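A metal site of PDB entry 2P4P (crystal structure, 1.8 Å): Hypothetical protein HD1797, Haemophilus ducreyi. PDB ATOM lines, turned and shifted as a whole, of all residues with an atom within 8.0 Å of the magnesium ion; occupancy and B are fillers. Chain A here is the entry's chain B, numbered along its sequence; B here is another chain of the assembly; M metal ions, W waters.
Water W1 lies within hydrogen-bond range of OD1 of Asp 69 of chain B (2.6 Å) and OD2 of Asp 76 of chain B (3.2 Å).
O of Asp 69 of chain A sits at hydrogen-bond distance from N of Asp 76 of chain A.
The magnesium ion is bound by the side-chain carboxylate of Glu 71 of chain A (2.1 Å), the side-chain carboxylate of Asp 69 of chain A (2.2 Å) and the backbone carbonyl oxygen of Thr 70 of chain A (2.4 Å).
The magnesium ion has three donor atoms within binding distance.
Slightly farther from the magnesium ion lies water W1 (2.8 Å).
Of the 14 residues printed, 3 come within 4 Å of the magnesium ion.
The nearest printed residue that does not touch the magnesium ion is Asp 69 of chain B (4.3 Å).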
ATOM      1  N   MLY A  54       3.435   4.968  12.559  1.00  0.00           N
ATOM      2  CA  MLY A  54       3.041   4.335  13.816  1.00  0.00           C
ATOM      3  CB  MLY A  54       2.681   5.469  14.786  1.00  0.00           C
ATOM      4  CG  MLY A  54       2.414   4.970  16.197  1.00  0.00           C
ATOM      5  CD  MLY A  54       2.257   6.099  17.222  1.00  0.00           C
ATOM      6  CE  MLY A  54       1.704   7.417  16.686  1.00  0.00           C
ATOM      7  NZ  MLY A  54       0.853   8.075  17.698  1.00  0.00           N
ATOM      8  CH1 MLY A  54       1.681   8.768  18.706  1.00  0.00           C
ATOM      9  CH2 MLY A  54      -0.037   9.062  17.066  1.00  0.00           C
ATOM     10  C   MLY A  54       1.859   3.415  13.612  1.00  0.00           C
ATOM     11  O   MLY A  54       0.913   3.760  12.892  1.00  0.00           O
ATOM     12  N   ILE A  68       6.363   1.546  16.749  1.00  0.00           N
ATOM     13  CA  ILE A  68       5.957   2.370  17.918  1.00  0.00           C
ATOM     14  C   ILE A  68       6.255   3.844  17.686  1.00  0.00           C
ATOM     15  O   ILE A  68       5.461   4.702  18.061  1.00  0.00           O
ATOM     16  CB  ILE A  68       6.645   1.870  19.231  1.00  0.00           C
ATOM     17  CG1 ILE A  68       6.216   0.427  19.546  1.00  0.00           C
ATOM     18  CG2 ILE A  68       6.384   2.834  20.447  1.00  0.00           C
ATOM     19  CD1 ILE A  68       4.659   0.193  19.791  1.00  0.00           C
ATOM     20  N   ASP A  69       7.400   4.154  17.068  1.00  0.00           N
ATOM     21  CA  ASP A  69       7.681   5.528  16.704  1.00  0.00           C
ATOM     22  C   ASP A  69       8.514   5.608  15.455  1.00  0.00           C
ATOM     23  O   ASP A  69       9.404   4.763  15.240  1.00  0.00           O
ATOM     24  CB  ASP A  69       8.396   6.261  17.855  1.00  0.00           C
ATOM     25  CG  ASP A  69       8.619   7.753  17.559  1.00  0.00           C
ATOM     26  OD1 ASP A  69       7.660   8.467  17.162  1.00  0.00           O
ATOM     27  OD2 ASP A  69       9.761   8.224  17.745  1.00  0.00           O
ATOM     28  N   THR A  70       8.215   6.602  14.623  1.00  0.00           N
ATOM     29  CA  THR A  70       9.112   6.991  13.554  1.00  0.00           C
ATOM     30  C   THR A  70       9.727   8.319  13.951  1.00  0.00           C
ATOM     31  O   THR A  70       9.033   9.224  14.466  1.00  0.00           O
ATOM     32  CB  THR A  70       8.424   7.181  12.191  1.00  0.00           C
ATOM     33  OG1 THR A  70       7.386   8.162  12.307  1.00  0.00           O
ATOM     34  CG2 THR A  70       7.845   5.854  11.683  1.00  0.00           C
ATOM     35  N   GLU A  71      11.008   8.450  13.691  1.00  0.00           N
ATOM     36  CA  GLU A  71      11.714   9.687  13.993  1.00  0.00           C
ATOM     37  C   GLU A  71      12.771   9.809  12.922  1.00  0.00           C
ATOM     38  O   GLU A  71      13.456   8.824  12.586  1.00  0.00           O
ATOM     39  CB  GLU A  71      12.324   9.632  15.409  1.00  0.00           C
ATOM     40  CG  GLU A  71      12.327  10.975  16.158  1.00  0.00           C
ATOM     41  CD  GLU A  71      11.016  11.268  16.911  1.00  0.00           C
ATOM     42  OE1 GLU A  71       9.962  10.678  16.562  1.00  0.00           O
ATOM     43  OE2 GLU A  71      11.026  12.091  17.868  1.00  0.00           O
ATOM     44  N   ASN A  72      12.851  11.001  12.327  1.00  0.00           N
ATOM     45  CA  ASN A  72      13.868  11.286  11.303  1.00  0.00           C
ATOM     46  C   ASN A  72      13.814  10.324  10.102  1.00  0.00           C
ATOM     47  O   ASN A  72      14.840   9.866   9.623  1.00  0.00           O
ATOM     48  CB  ASN A  72      15.269  11.228  11.953  1.00  0.00           C
ATOM     49  CG  ASN A  72      16.362  11.672  11.018  1.00  0.00           C
ATOM     50  OD1 ASN A  72      16.221  12.661  10.271  1.00  0.00           O
ATOM     51  ND2 ASN A  72      17.481  10.943  11.047  1.00  0.00           N
ATOM     52  N   ARG A  74      13.063   7.367   9.728  1.00  0.00           N
ATOM     53  CA  ARG A  74      13.351   5.966   9.968  1.00  0.00           C
ATOM     54  C   ARG A  74      12.399   5.439  11.049  1.00  0.00           C
ATOM     55  O   ARG A  74      11.738   6.209  11.757  1.00  0.00           O
ATOM     56  CB  ARG A  74      14.823   5.759  10.381  1.00  0.00           C
ATOM     57  CG  ARG A  74      15.876   6.342   9.435  1.00  0.00           C
ATOM     58  CD  ARG A  74      16.220   5.450   8.219  1.00  0.00           C
ATOM     59  NE  ARG A  74      17.004   4.257   8.560  1.00  0.00           N
ATOM     60  CZ  ARG A  74      17.832   3.633   7.720  1.00  0.00           C
ATOM     61  NH1 ARG A  74      17.992   4.094   6.479  1.00  0.00           N
ATOM     62  NH2 ARG A  74      18.508   2.558   8.099  1.00  0.00           N
ATOM     63  N   ASP A  76      11.928   4.278  14.477  1.00  0.00           N
ATOM     64  CA  ASP A  76      12.831   4.609  15.580  1.00  0.00           C
ATOM     65  C   ASP A  76      12.743   3.554  16.682  1.00  0.00           C
ATOM     66  O   ASP A  76      13.774   3.099  17.175  1.00  0.00           O
ATOM     67  CB  ASP A  76      12.534   5.989  16.151  1.00  0.00           C
ATOM     68  CG  ASP A  76      13.602   6.449  17.131  1.00  0.00           C
ATOM     69  OD1 ASP A  76      14.802   6.515  16.745  1.00  0.00           O
ATOM     70  OD2 ASP A  76      13.255   6.724  18.274  1.00  0.00           O
ATOM     71  N   ILE B  68      10.053   6.832  25.659  1.00  0.00           N
ATOM     72  CA  ILE B  68      10.214   6.148  24.379  1.00  0.00           C
ATOM     73  C   ILE B  68      10.304   7.182  23.264  1.00  0.00           C
ATOM     74  O   ILE B  68      11.158   7.098  22.372  1.00  0.00           O
ATOM     75  CB  ILE B  68       9.109   5.062  24.150  1.00  0.00           C
ATOM     76  CG1 ILE B  68       9.302   3.915  25.155  1.00  0.00           C
ATOM     77  CG2 ILE B  68       9.065   4.559  22.660  1.00  0.00           C
ATOM     78  CD1 ILE B  68      10.785   3.389  25.269  1.00  0.00           C
ATOM     79  N   ASP B  69       9.425   8.169  23.325  1.00  0.00           N
ATOM     80  CA  ASP B  69       9.506   9.302  22.412  1.00  0.00           C
ATOM     81  C   ASP B  69       8.844  10.572  22.957  1.00  0.00           C
ATOM     82  O   ASP B  69       7.924  10.519  23.780  1.00  0.00           O
ATOM     83  CB  ASP B  69       8.955   8.907  21.038  1.00  0.00           C
ATOM     84  CG  ASP B  69       7.441   8.851  21.000  1.00  0.00           C
ATOM     85  OD1 ASP B  69       6.852   9.722  20.336  1.00  0.00           O
ATOM     86  OD2 ASP B  69       6.816   7.948  21.615  1.00  0.00           O
ATOM     87  N   THR B  70       9.336  11.718  22.490  1.00  0.00           N
ATOM     88  CA  THR B  70       8.686  12.988  22.741  1.00  0.00           C
ATOM     89  C   THR B  70       8.024  13.463  21.430  1.00  0.00           C
ATOM     90  O   THR B  70       8.438  13.078  20.334  1.00  0.00           O
ATOM     91  CB  THR B  70       9.664  14.079  23.269  1.00  0.00           C
ATOM     92  OG1 THR B  70      10.605  14.434  22.249  1.00  0.00           O
ATOM     93  CG2 THR B  70      10.413  13.599  24.549  1.00  0.00           C
ATOM     94  N   GLU B  71       6.953  14.218  21.573  1.00  0.00           N
ATOM     95  CA  GLU B  71       6.365  14.912  20.451  1.00  0.00           C
ATOM     96  C   GLU B  71       5.608  16.126  20.979  1.00  0.00           C
ATOM     97  O   GLU B  71       5.003  16.086  22.069  1.00  0.00           O
ATOM     98  CB  GLU B  71       5.501  13.996  19.591  1.00  0.00           C
ATOM     99  CG  GLU B  71       4.138  13.584  20.169  1.00  0.00           C
ATOM    100  CD  GLU B  71       3.096  13.345  19.094  1.00  0.00           C
ATOM    101  OE1 GLU B  71       2.112  12.610  19.362  1.00  0.00           O
ATOM    102  OE2 GLU B  71       3.252  13.878  17.973  1.00  0.00           O
ATOM    103  N   ASP B  76       5.474  11.631  24.848  1.00  0.00           N
ATOM    104  CA  ASP B  76       4.382  11.051  24.074  1.00  0.00           C
ATOM    105  C   ASP B  76       4.121   9.603  24.554  1.00  0.00           C
ATOM    106  O   ASP B  76       2.979   9.237  24.901  1.00  0.00           O
ATOM    107  CB  ASP B  76       4.784  11.135  22.583  1.00  0.00           C
ATOM    108  CG  ASP B  76       3.824  10.435  21.654  1.00  0.00           C
ATOM    109  OD1 ASP B  76       2.596  10.538  21.827  1.00  0.00           O
ATOM    110  OD2 ASP B  76       4.324   9.792  20.712  1.00  0.00           O
ATOM    111  N   GLN B  77       5.186   8.803  24.571  1.00  0.00           N
ATOM    112  CA  GLN B  77       5.133   7.422  25.090  1.00  0.00           C
ATOM    113  C   GLN B  77       6.264   7.119  26.039  1.00  0.00           C
ATOM    114  O   GLN B  77       7.391   7.550  25.820  1.00  0.00           O
ATOM    115  CB  GLN B  77       5.191   6.411  23.967  1.00  0.00           C
ATOM    116  CG  GLN B  77       3.955   6.396  23.112  1.00  0.00           C
ATOM    117  CD  GLN B  77       4.073   5.412  21.987  1.00  0.00           C
ATOM    118  OE1 GLN B  77       3.307   4.471  21.896  1.00  0.00           O
ATOM    119  NE2 GLN B  77       5.043   5.611  21.125  1.00  0.00           N
HETATM  120 MG    MG M   1       7.945  10.452  16.272  1.00  0.00          MG
HETATM  121  O   HOH W   1       5.940  10.954  18.218  1.00  0.00           O
